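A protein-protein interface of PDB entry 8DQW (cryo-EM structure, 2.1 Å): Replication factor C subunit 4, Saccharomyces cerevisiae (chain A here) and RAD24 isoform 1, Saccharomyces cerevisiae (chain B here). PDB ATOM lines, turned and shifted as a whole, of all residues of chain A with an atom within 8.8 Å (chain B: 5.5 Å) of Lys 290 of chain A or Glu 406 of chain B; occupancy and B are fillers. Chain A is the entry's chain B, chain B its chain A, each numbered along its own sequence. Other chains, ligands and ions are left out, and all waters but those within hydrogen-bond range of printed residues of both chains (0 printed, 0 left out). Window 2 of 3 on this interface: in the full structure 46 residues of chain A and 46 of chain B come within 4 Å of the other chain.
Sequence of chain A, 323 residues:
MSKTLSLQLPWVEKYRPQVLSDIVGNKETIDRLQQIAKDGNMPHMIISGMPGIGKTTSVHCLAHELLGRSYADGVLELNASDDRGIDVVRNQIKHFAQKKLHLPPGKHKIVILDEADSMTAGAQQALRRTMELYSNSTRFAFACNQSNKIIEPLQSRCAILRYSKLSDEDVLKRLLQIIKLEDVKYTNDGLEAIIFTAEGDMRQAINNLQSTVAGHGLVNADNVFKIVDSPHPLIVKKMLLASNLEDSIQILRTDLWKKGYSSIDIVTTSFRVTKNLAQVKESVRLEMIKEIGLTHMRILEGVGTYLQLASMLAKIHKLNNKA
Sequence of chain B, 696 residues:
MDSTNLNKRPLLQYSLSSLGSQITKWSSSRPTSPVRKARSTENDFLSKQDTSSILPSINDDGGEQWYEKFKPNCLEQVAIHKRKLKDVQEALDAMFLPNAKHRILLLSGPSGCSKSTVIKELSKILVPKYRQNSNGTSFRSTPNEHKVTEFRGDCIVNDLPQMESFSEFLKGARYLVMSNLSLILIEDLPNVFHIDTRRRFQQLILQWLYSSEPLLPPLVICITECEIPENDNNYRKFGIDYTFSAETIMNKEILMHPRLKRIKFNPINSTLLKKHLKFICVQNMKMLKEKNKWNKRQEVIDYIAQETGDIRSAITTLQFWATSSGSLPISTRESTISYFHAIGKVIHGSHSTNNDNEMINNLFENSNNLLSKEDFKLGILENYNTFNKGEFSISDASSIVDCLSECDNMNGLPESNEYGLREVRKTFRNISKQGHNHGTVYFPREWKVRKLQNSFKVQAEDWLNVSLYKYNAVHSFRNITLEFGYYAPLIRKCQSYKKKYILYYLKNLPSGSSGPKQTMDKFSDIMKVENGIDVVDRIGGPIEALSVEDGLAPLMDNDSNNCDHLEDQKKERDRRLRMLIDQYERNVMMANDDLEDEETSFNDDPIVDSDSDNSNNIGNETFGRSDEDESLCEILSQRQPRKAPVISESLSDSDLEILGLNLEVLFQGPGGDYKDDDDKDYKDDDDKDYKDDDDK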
ATOM      1  N   PHE A 271     -18.712   0.916  14.301  1.00  0.00           N
ATOM      2  CA  PHE A 271     -17.741   0.912  13.208  1.00  0.00           C
ATOM      3  C   PHE A 271     -18.399   1.349  11.902  1.00  0.00           C
ATOM      4  O   PHE A 271     -17.874   2.210  11.178  1.00  0.00           O
ATOM      5  CB  PHE A 271     -17.116  -0.476  13.069  1.00  0.00           C
ATOM      6  CG  PHE A 271     -16.224  -0.627  11.867  1.00  0.00           C
ATOM      7  CD1 PHE A 271     -15.231   0.301  11.601  1.00  0.00           C
ATOM      8  CD2 PHE A 271     -16.367  -1.709  11.013  1.00  0.00           C
ATOM      9  CE1 PHE A 271     -14.406   0.161  10.499  1.00  0.00           C
ATOM     10  CE2 PHE A 271     -15.543  -1.855   9.912  1.00  0.00           C
ATOM     11  CZ  PHE A 271     -14.562  -0.919   9.654  1.00  0.00           C
ATOM     12  N   THR A 274     -19.102   5.140  12.084  1.00  0.00           N
ATOM     13  CA  THR A 274     -17.881   5.933  12.021  1.00  0.00           C
ATOM     14  C   THR A 274     -17.312   5.957  10.613  1.00  0.00           C
ATOM     15  O   THR A 274     -16.691   6.946  10.211  1.00  0.00           O
ATOM     16  CB  THR A 274     -16.846   5.383  13.005  1.00  0.00           C
ATOM     17  OG1 THR A 274     -17.298   5.593  14.349  1.00  0.00           O
ATOM     18  CG2 THR A 274     -15.501   6.073  12.816  1.00  0.00           C
ATOM     19  N   SER A 283      -7.735  11.906  10.579  1.00  0.00           N
ATOM     20  CA  SER A 283      -6.936  11.370  11.677  1.00  0.00           C
ATOM     21  C   SER A 283      -7.826  10.919  12.830  1.00  0.00           C
ATOM     22  O   SER A 283      -7.681   9.803  13.350  1.00  0.00           O
ATOM     23  CB  SER A 283      -5.934  12.424  12.152  1.00  0.00           C
ATOM     24  OG  SER A 283      -5.112  11.915  13.187  1.00  0.00           O
ATOM     25  N   VAL A 284      -8.765  11.776  13.234  1.00  0.00           N
ATOM     26  CA  VAL A 284      -9.680  11.425  14.315  1.00  0.00           C
ATOM     27  C   VAL A 284     -10.501  10.200  13.932  1.00  0.00           C
ATOM     28  O   VAL A 284     -10.717   9.299  14.750  1.00  0.00           O
ATOM     29  CB  VAL A 284     -10.578  12.627  14.661  1.00  0.00           C
ATOM     30  CG1 VAL A 284     -11.625  12.234  15.690  1.00  0.00           C
ATOM     31  CG2 VAL A 284      -9.737  13.791  15.167  1.00  0.00           C
ATOM     32  N   ARG A 285     -10.974  10.151  12.685  1.00  0.00           N
ATOM     33  CA  ARG A 285     -11.789   9.024  12.245  1.00  0.00           C
ATOM     34  C   ARG A 285     -11.014   7.715  12.327  1.00  0.00           C
ATOM     35  O   ARG A 285     -11.525   6.707  12.831  1.00  0.00           O
ATOM     36  CB  ARG A 285     -12.279   9.265  10.818  1.00  0.00           C
ATOM     37  CG  ARG A 285     -13.345   8.288  10.352  1.00  0.00           C
ATOM     38  CD  ARG A 285     -13.271   8.069   8.853  1.00  0.00           C
ATOM     39  NE  ARG A 285     -13.487   9.311   8.121  1.00  0.00           N
ATOM     40  CZ  ARG A 285     -14.654   9.932   8.027  1.00  0.00           C
ATOM     41  NH1 ARG A 285     -15.744   9.441   8.593  1.00  0.00           N
ATOM     42  NH2 ARG A 285     -14.731  11.071   7.346  1.00  0.00           N
ATOM     43  N   LEU A 286      -9.775   7.707  11.831  1.00  0.00           N
ATOM     44  CA  LEU A 286      -9.009   6.465  11.823  1.00  0.00           C
ATOM     45  C   LEU A 286      -8.630   6.046  13.241  1.00  0.00           C
ATOM     46  O   LEU A 286      -8.609   4.849  13.553  1.00  0.00           O
ATOM     47  CB  LEU A 286      -7.772   6.611  10.933  1.00  0.00           C
ATOM     48  CG  LEU A 286      -6.557   7.375  11.461  1.00  0.00           C
ATOM     49  CD1 LEU A 286      -5.589   6.416  12.132  1.00  0.00           C
ATOM     50  CD2 LEU A 286      -5.864   8.138  10.339  1.00  0.00           C
ATOM     51  N   GLU A 287      -8.354   7.011  14.124  1.00  0.00           N
ATOM     52  CA  GLU A 287      -8.096   6.659  15.519  1.00  0.00           C
ATOM     53  C   GLU A 287      -9.339   6.072  16.187  1.00  0.00           C
ATOM     54  O   GLU A 287      -9.244   5.102  16.954  1.00  0.00           O
ATOM     55  CB  GLU A 287      -7.602   7.881  16.290  1.00  0.00           C
ATOM     56  CG  GLU A 287      -6.102   7.874  16.563  1.00  0.00           C
ATOM     57  CD  GLU A 287      -5.270   7.880  15.301  1.00  0.00           C
ATOM     58  OE1 GLU A 287      -5.806   8.263  14.242  1.00  0.00           O
ATOM     59  OE2 GLU A 287      -4.082   7.501  15.368  1.00  0.00           O
ATOM     60  N   MET A 288     -10.513   6.647  15.915  1.00  0.00           N
ATOM     61  CA  MET A 288     -11.747   6.080  16.452  1.00  0.00           C
ATOM     62  C   MET A 288     -11.963   4.668  15.929  1.00  0.00           C
ATOM     63  O   MET A 288     -12.412   3.785  16.668  1.00  0.00           O
ATOM     64  CB  MET A 288     -12.941   6.967  16.096  1.00  0.00           C
ATOM     65  CG  MET A 288     -12.886   8.365  16.687  1.00  0.00           C
ATOM     66  SD  MET A 288     -13.937   9.539  15.807  1.00  0.00           S
ATOM     67  CE  MET A 288     -15.463   8.613  15.669  1.00  0.00           C
ATOM     68  N   ILE A 289     -11.655   4.440  14.651  1.00  0.00           N
ATOM     69  CA  ILE A 289     -11.769   3.100  14.083  1.00  0.00           C
ATOM     70  C   ILE A 289     -10.834   2.138  14.805  1.00  0.00           C
ATOM     71  O   ILE A 289     -11.200   0.993  15.091  1.00  0.00           O
ATOM     72  CB  ILE A 289     -11.485   3.138  12.569  1.00  0.00           C
ATOM     73  CG1 ILE A 289     -12.659   3.789  11.831  1.00  0.00           C
ATOM     74  CG2 ILE A 289     -11.226   1.729  12.043  1.00  0.00           C
ATOM     75  CD1 ILE A 289     -12.397   4.050  10.361  1.00  0.00           C
ATOM     76  N   LYS A 290      -9.612   2.582  15.098  1.00  0.00           N
ATOM     77  CA  LYS A 290      -8.671   1.733  15.827  1.00  0.00           C
ATOM     78  C   LYS A 290      -9.224   1.358  17.198  1.00  0.00           C
ATOM     79  O   LYS A 290      -9.168   0.190  17.610  1.00  0.00           O
ATOM     80  CB  LYS A 290      -7.327   2.450  15.967  1.00  0.00           C
ATOM     81  CG  LYS A 290      -6.258   1.654  16.708  1.00  0.00           C
ATOM     82  CD  LYS A 290      -5.136   2.556  17.196  1.00  0.00           C
ATOM     83  CE  LYS A 290      -4.069   1.766  17.934  1.00  0.00           C
ATOM     84  NZ  LYS A 290      -3.103   2.650  18.640  1.00  0.00           N
ATOM     85  N   GLU A 291      -9.754   2.342  17.928  1.00  0.00           N
ATOM     86  CA  GLU A 291     -10.286   2.055  19.257  1.00  0.00           C
ATOM     87  C   GLU A 291     -11.484   1.114  19.180  1.00  0.00           C
ATOM     88  O   GLU A 291     -11.620   0.194  19.999  1.00  0.00           O
ATOM     89  CB  GLU A 291     -10.667   3.356  19.966  1.00  0.00           C
ATOM     90  CG  GLU A 291      -9.480   4.236  20.345  1.00  0.00           C
ATOM     91  CD  GLU A 291      -8.442   3.511  21.187  1.00  0.00           C
ATOM     92  OE1 GLU A 291      -8.766   2.447  21.754  1.00  0.00           O
ATOM     93  OE2 GLU A 291      -7.300   4.006  21.279  1.00  0.00           O
ATOM     94  N   ILE A 292     -12.362   1.327  18.197  1.00  0.00           N
ATOM     95  CA  ILE A 292     -13.511   0.446  18.017  1.00  0.00           C
ATOM     96  C   ILE A 292     -13.047  -0.973  17.721  1.00  0.00           C
ATOM     97  O   ILE A 292     -13.605  -1.944  18.240  1.00  0.00           O
ATOM     98  CB  ILE A 292     -14.429   0.989  16.906  1.00  0.00           C
ATOM     99  CG1 ILE A 292     -15.188   2.221  17.403  1.00  0.00           C
ATOM    100  CG2 ILE A 292     -15.404  -0.085  16.440  1.00  0.00           C
ATOM    101  CD1 ILE A 292     -15.762   3.077  16.292  1.00  0.00           C
ATOM    102  N   GLY A 293     -12.024  -1.117  16.877  1.00  0.00           N
ATOM    103  CA  GLY A 293     -11.507  -2.442  16.575  1.00  0.00           C
ATOM    104  C   GLY A 293     -10.924  -3.133  17.792  1.00  0.00           C
ATOM    105  O   GLY A 293     -11.126  -4.332  17.994  1.00  0.00           O
ATOM    106  N   LEU A 294     -10.183  -2.390  18.618  1.00  0.00           N
ATOM    107  CA  LEU A 294      -9.629  -2.989  19.830  1.00  0.00           C
ATOM    108  C   LEU A 294     -10.740  -3.439  20.776  1.00  0.00           C
ATOM    109  O   LEU A 294     -10.680  -4.539  21.347  1.00  0.00           O
ATOM    110  CB  LEU A 294      -8.693  -2.000  20.526  1.00  0.00           C
ATOM    111  CG  LEU A 294      -7.410  -1.662  19.758  1.00  0.00           C
ATOM    112  CD1 LEU A 294      -6.774  -0.391  20.300  1.00  0.00           C
ATOM    113  CD2 LEU A 294      -6.422  -2.823  19.805  1.00  0.00           C
ATOM    114  N   THR A 295     -11.775  -2.610  20.942  1.00  0.00           N
ATOM    115  CA  THR A 295     -12.892  -3.000  21.797  1.00  0.00           C
ATOM    116  C   THR A 295     -13.620  -4.214  21.226  1.00  0.00           C
ATOM    117  O   THR A 295     -14.069  -5.089  21.975  1.00  0.00           O
ATOM    118  CB  THR A 295     -13.855  -1.826  21.975  1.00  0.00           C
ATOM    119  OG1 THR A 295     -13.256  -0.839  22.824  1.00  0.00           O
ATOM    120  CG2 THR A 295     -15.159  -2.291  22.605  1.00  0.00           C
ATOM    121  N   HIS A 296     -13.754  -4.276  19.899  1.00  0.00           N
ATOM    122  CA  HIS A 296     -14.367  -5.436  19.261  1.00  0.00           C
ATOM    123  C   HIS A 296     -13.550  -6.696  19.517  1.00  0.00           C
ATOM    124  O   HIS A 296     -14.108  -7.769  19.777  1.00  0.00           O
ATOM    125  CB  HIS A 296     -14.509  -5.177  17.760  1.00  0.00           C
ATOM    126  CG  HIS A 296     -15.240  -6.252  17.019  1.00  0.00           C
ATOM    127  ND1 HIS A 296     -15.385  -6.241  15.648  1.00  0.00           N
ATOM    128  CD2 HIS A 296     -15.868  -7.371  17.453  1.00  0.00           C
ATOM    129  CE1 HIS A 296     -16.068  -7.306  15.270  1.00  0.00           C
ATOM    130  NE2 HIS A 296     -16.372  -8.010  16.346  1.00  0.00           N
ATOM    131  N   MET A 297     -12.224  -6.586  19.439  1.00  0.00           N
ATOM    132  CA  MET A 297     -11.368  -7.720  19.769  1.00  0.00           C
ATOM    133  C   MET A 297     -11.606  -8.175  21.201  1.00  0.00           C
ATOM    134  O   MET A 297     -11.710  -9.376  21.472  1.00  0.00           O
ATOM    135  CB  MET A 297      -9.900  -7.346  19.572  1.00  0.00           C
ATOM    136  CG  MET A 297      -8.935  -8.504  19.769  1.00  0.00           C
ATOM    137  SD  MET A 297      -7.229  -8.073  19.372  1.00  0.00           S
ATOM    138  CE  MET A 297      -6.908  -6.798  20.589  1.00  0.00           C
ATOM    139  N   MET A 312     -14.358   2.456  25.715  1.00  0.00           N
ATOM    140  CA  MET A 312     -14.260   2.825  24.306  1.00  0.00           C
ATOM    141  C   MET A 312     -14.746   4.253  24.086  1.00  0.00           C
ATOM    142  O   MET A 312     -14.104   5.038  23.375  1.00  0.00           O
ATOM    143  CB  MET A 312     -15.071   1.844  23.456  1.00  0.00           C
ATOM    144  CG  MET A 312     -14.943   2.050  21.953  1.00  0.00           C
ATOM    145  SD  MET A 312     -16.222   1.189  21.013  1.00  0.00           S
ATOM    146  CE  MET A 312     -17.684   2.121  21.473  1.00  0.00           C
ATOM    147  N   LYS A 315     -12.154   6.716  25.414  1.00  0.00           N
ATOM    148  CA  LYS A 315     -11.028   6.869  24.497  1.00  0.00           C
ATOM    149  C   LYS A 315     -11.410   7.723  23.293  1.00  0.00           C
ATOM    150  O   LYS A 315     -10.638   8.592  22.865  1.00  0.00           O
ATOM    151  CB  LYS A 315     -10.533   5.497  24.040  1.00  0.00           C
ATOM    152  CG  LYS A 315      -9.361   4.961  24.848  1.00  0.00           C
ATOM    153  CD  LYS A 315      -9.126   3.482  24.583  1.00  0.00           C
ATOM    154  CE  LYS A 315      -8.711   2.744  25.844  1.00  0.00           C
ATOM    155  NZ  LYS A 315      -7.487   3.334  26.452  1.00  0.00           N
ATOM    156  N   ILE A 316     -12.602   7.493  22.735  1.00  0.00           N
ATOM    157  CA  ILE A 316     -13.039   8.290  21.592  1.00  0.00           C
ATOM    158  C   ILE A 316     -13.124   9.759  21.977  1.00  0.00           C
ATOM    159  O   ILE A 316     -12.682  10.641  21.227  1.00  0.00           O
ATOM    160  CB  ILE A 316     -14.385   7.770  21.054  1.00  0.00           C
ATOM    161  CG1 ILE A 316     -14.169   6.509  20.215  1.00  0.00           C
ATOM    162  CG2 ILE A 316     -15.086   8.854  20.236  1.00  0.00           C
ATOM    163  CD1 ILE A 316     -15.451   5.813  19.800  1.00  0.00           C
ATOM    164  N   LEU A 319      -9.790  11.324  22.142  1.00  0.00           N
ATOM    165  CA  LEU A 319      -9.274  11.621  20.812  1.00  0.00           C
ATOM    166  C   LEU A 319      -9.912  12.879  20.239  1.00  0.00           C
ATOM    167  O   LEU A 319      -9.236  13.683  19.587  1.00  0.00           O
ATOM    168  CB  LEU A 319      -9.499  10.432  19.880  1.00  0.00           C
ATOM    169  CG  LEU A 319      -8.436   9.352  20.083  1.00  0.00           C
ATOM    170  CD1 LEU A 319      -9.047   7.954  20.031  1.00  0.00           C
ATOM    171  CD2 LEU A 319      -7.294   9.504  19.100  1.00  0.00           C
ATOM    172  N   VAL B 401       5.119   2.009  10.073  1.00  0.00           N
ATOM    173  CA  VAL B 401       5.476   0.642  10.441  1.00  0.00           C
ATOM    174  C   VAL B 401       4.856   0.269  11.783  1.00  0.00           C
ATOM    175  O   VAL B 401       4.410  -0.867  11.975  1.00  0.00           O
ATOM    176  CB  VAL B 401       7.005   0.470  10.449  1.00  0.00           C
ATOM    177  CG1 VAL B 401       7.381  -0.929  10.910  1.00  0.00           C
ATOM    178  CG2 VAL B 401       7.575   0.733   9.063  1.00  0.00           C
ATOM    179  N   ASP B 402       4.826   1.206  12.733  1.00  0.00           N
ATOM    180  CA  ASP B 402       4.191   0.930  14.016  1.00  0.00           C
ATOM    181  C   ASP B 402       2.698   0.687  13.840  1.00  0.00           C
ATOM    182  O   ASP B 402       2.121  -0.191  14.493  1.00  0.00           O
ATOM    183  CB  ASP B 402       4.436   2.089  14.982  1.00  0.00           C
ATOM    184  CG  ASP B 402       3.842   1.840  16.354  1.00  0.00           C
ATOM    185  OD1 ASP B 402       3.819   0.669  16.789  1.00  0.00           O
ATOM    186  OD2 ASP B 402       3.401   2.813  16.998  1.00  0.00           O
ATOM    187  N   CYS B 403       2.057   1.456  12.959  1.00  0.00           N
ATOM    188  CA  CYS B 403       0.647   1.226  12.671  1.00  0.00           C
ATOM    189  C   CYS B 403       0.423  -0.166  12.090  1.00  0.00           C
ATOM    190  O   CYS B 403      -0.510  -0.872  12.491  1.00  0.00           O
ATOM    191  CB  CYS B 403       0.139   2.303  11.715  1.00  0.00           C
ATOM    192  SG  CYS B 403      -1.327   1.841  10.800  1.00  0.00           S
ATOM    193  N   LEU B 404       1.272  -0.580  11.145  1.00  0.00           N
ATOM    194  CA  LEU B 404       1.129  -1.917  10.571  1.00  0.00           C
ATOM    195  C   LEU B 404       1.359  -2.997  11.625  1.00  0.00           C
ATOM    196  O   LEU B 404       0.658  -4.018  11.646  1.00  0.00           O
ATOM    197  CB  LEU B 404       2.098  -2.094   9.401  1.00  0.00           C
ATOM    198  CG  LEU B 404       1.865  -1.178   8.196  1.00  0.00           C
ATOM    199  CD1 LEU B 404       3.014  -1.296   7.205  1.00  0.00           C
ATOM    200  CD2 LEU B 404       0.539  -1.490   7.516  1.00  0.00           C
ATOM    201  N   SER B 405       2.339  -2.792  12.506  1.00  0.00           N
ATOM    202  CA  SER B 405       2.591  -3.752  13.575  1.00  0.00           C
ATOM    203  C   SER B 405       1.382  -3.876  14.493  1.00  0.00           C
ATOM    204  O   SER B 405       0.993  -4.985  14.875  1.00  0.00           O
ATOM    205  CB  SER B 405       3.830  -3.335  14.366  1.00  0.00           C
ATOM    206  OG  SER B 405       4.071  -4.210  15.453  1.00  0.00           O
ATOM    207  N   GLU B 406       0.771  -2.745  14.853  1.00  0.00           N
ATOM    208  CA  GLU B 406      -0.436  -2.789  15.674  1.00  0.00           C
ATOM    209  C   GLU B 406      -1.562  -3.516  14.949  1.00  0.00           C
ATOM    210  O   GLU B 406      -2.287  -4.315  15.553  1.00  0.00           O
ATOM    211  CB  GLU B 406      -0.871  -1.373  16.048  1.00  0.00           C
ATOM    212  CG  GLU B 406      -0.004  -0.715  17.106  1.00  0.00           C
ATOM    213  CD  GLU B 406      -0.757   0.319  17.922  1.00  0.00           C
ATOM    214  OE1 GLU B 406      -1.775  -0.041  18.547  1.00  0.00           O
ATOM    215  OE2 GLU B 406      -0.328   1.492  17.936  1.00  0.00           O
ATOM    216  N   CYS B 407      -1.722  -3.252  13.650  1.00  0.00           N
ATOM    217  CA  CYS B 407      -2.772  -3.914  12.884  1.00  0.00           C
ATOM    218  C   CYS B 407      -2.560  -5.420  12.829  1.00  0.00           C
ATOM    219  O   CYS B 407      -3.533  -6.184  12.795  1.00  0.00           O
ATOM    220  CB  CYS B 407      -2.834  -3.336  11.470  1.00  0.00           C
ATOM    221  SG  CYS B 407      -3.556  -1.693  11.362  1.00  0.00           S
ATOM    222  N   ASP B 408      -1.303  -5.869  12.811  1.00  0.00           N
ATOM    223  CA  ASP B 408      -1.030  -7.303  12.777  1.00  0.00           C
ATOM    224  C   ASP B 408      -1.525  -8.019  14.030  1.00  0.00           C
ATOM    225  O   ASP B 408      -1.632  -9.249  14.025  1.00  0.00           O
ATOM    226  CB  ASP B 408       0.469  -7.555  12.601  1.00  0.00           C
ATOM    227  CG  ASP B 408       0.823  -9.031  12.657  1.00  0.00           C
ATOM    228  OD1 ASP B 408       0.339  -9.794  11.796  1.00  0.00           O
ATOM    229  OD2 ASP B 408       1.579  -9.429  13.567  1.00  0.00           O
ATOM    230  N   ASN B 409      -1.826  -7.283  15.099  1.00  0.00           N
ATOM    231  CA  ASN B 409      -2.263  -7.865  16.361  1.00  0.00           C
ATOM    232  C   ASN B 409      -3.779  -7.858  16.523  1.00  0.00           C
ATOM    233  O   ASN B 409      -4.274  -8.118  17.625  1.00  0.00           O
ATOM    234  CB  ASN B 409      -1.618  -7.116  17.532  1.00  0.00           C
ATOM    235  CG  ASN B 409      -0.237  -7.647  17.890  1.00  0.00           C
ATOM    236  OD1 ASN B 409       0.211  -7.506  19.027  1.00  0.00           O
ATOM    237  ND2 ASN B 409       0.446  -8.251  16.921  1.00  0.00           N
ATOM    238  N   MET B 410      -4.526  -7.572  15.455  1.00  0.00           N
ATOM    239  CA  MET B 410      -5.969  -7.385  15.537  1.00  0.00           C
ATOM    240  C   MET B 410      -6.753  -8.568  14.972  1.00  0.00           C
ATOM    241  O   MET B 410      -7.937  -8.423  14.650  1.00  0.00           O
ATOM    242  CB  MET B 410      -6.363  -6.096  14.818  1.00  0.00           C
ATOM    243  CG  MET B 410      -5.774  -4.847  15.449  1.00  0.00           C
ATOM    244  SD  MET B 410      -6.496  -3.326  14.806  1.00  0.00           S
ATOM    245  CE  MET B 410      -7.089  -2.573  16.319  1.00  0.00           C
ATOM    246  N   TYR B 419      -7.871   0.765   9.379  1.00  0.00           N
ATOM    247  CA  TYR B 419      -6.996   1.653  10.136  1.00  0.00           C
ATOM    248  C   TYR B 419      -5.612   1.727   9.507  1.00  0.00           C
ATOM    249  O   TYR B 419      -5.039   2.816   9.382  1.00  0.00           O
ATOM    250  CB  TYR B 419      -6.915   1.175  11.588  1.00  0.00           C
ATOM    251  CG  TYR B 419      -5.741   1.715  12.377  1.00  0.00           C
ATOM    252  CD1 TYR B 419      -5.538   3.081  12.521  1.00  0.00           C
ATOM    253  CD2 TYR B 419      -4.844   0.855  12.996  1.00  0.00           C
ATOM    254  CE1 TYR B 419      -4.467   3.572  13.247  1.00  0.00           C
ATOM    255  CE2 TYR B 419      -3.776   1.335  13.725  1.00  0.00           C
ATOM    256  CZ  TYR B 419      -3.589   2.694  13.846  1.00  0.00           C
ATOM    257  OH  TYR B 419      -2.523   3.175  14.572  1.00  0.00           O
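The side-chain carboxylate of Glu 406 of chain B lies within salt-bridge range of the side-chain amino group of Lys 290 of chain A, at 3.0 Å. The backbone carbonyl oxygen (O) of Asn 409 of chain B lies close to the side-chain sulfur (SD) of Met 297 of chain A.
Hydrophobic or aromatic side chains of chain A that line the printed part of chain B: Leu 286, Leu 294 and Met 297. Of the 11 printed residues of chain B, 4 touch a printed residue of chain A. Printed residues of chain B that touch a printed residue of chain A: Glu 406, Asn 409, Met 410 and Tyr 419. Among the printed residues, Asp or Glu carboxylates within 4 Å of a Lys or Arg side-chain nitrogen of the other chain: Lys 290 of chain A with Glu 406 of chain B (3.0 Å).
Of chain B, only Glu 406 (3.0 Å), Met 410 (3.7 Å) and Tyr 419 (3.7 Å) come within 4 Å of Lys 290 of chain A. Glu 406 of chain B touches one residue of chain A. Ser 405 of chain B touches none of the printed residues of chain A. Cys 407 of chain B touches none of the printed residues of chain A. Of the printed residues of chain B, Met 297 of chain A touches Asn 409. Printed residues of chain A within 4 Å of Tyr 419 of chain B: Leu 286 (3.3 Å) and Lys 290 (3.7 Å). Of the printed residues of chain B, Leu 286 of chain A touches Tyr 419. Of the printed residues of chain A, Met 410 of chain B touches Lys 290 (3.7 Å) and Leu 294 (3.6 Å). The nearest printed residue of chain B that does not touch Lys 290 of chain A is Asp 402 of chain B (6.7 Å). The nearest residue of chain A that does not touch Glu 406 of chain B is Leu 294 of chain A (5.3 Å). The nearest printed residue of chain B that does not touch Leu 294 of chain A is Glu 406 of chain B (5.3 Å).
Among the printed residues, merely in contact across the chains: Leu 286 of chain A with Tyr 419 of chain B, Leu 294 of chain A with Met 410 of chain B, Lys 290 of chain A with Met 410 of chain B and Lys 290 of chain A with Tyr 419 of chain B.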
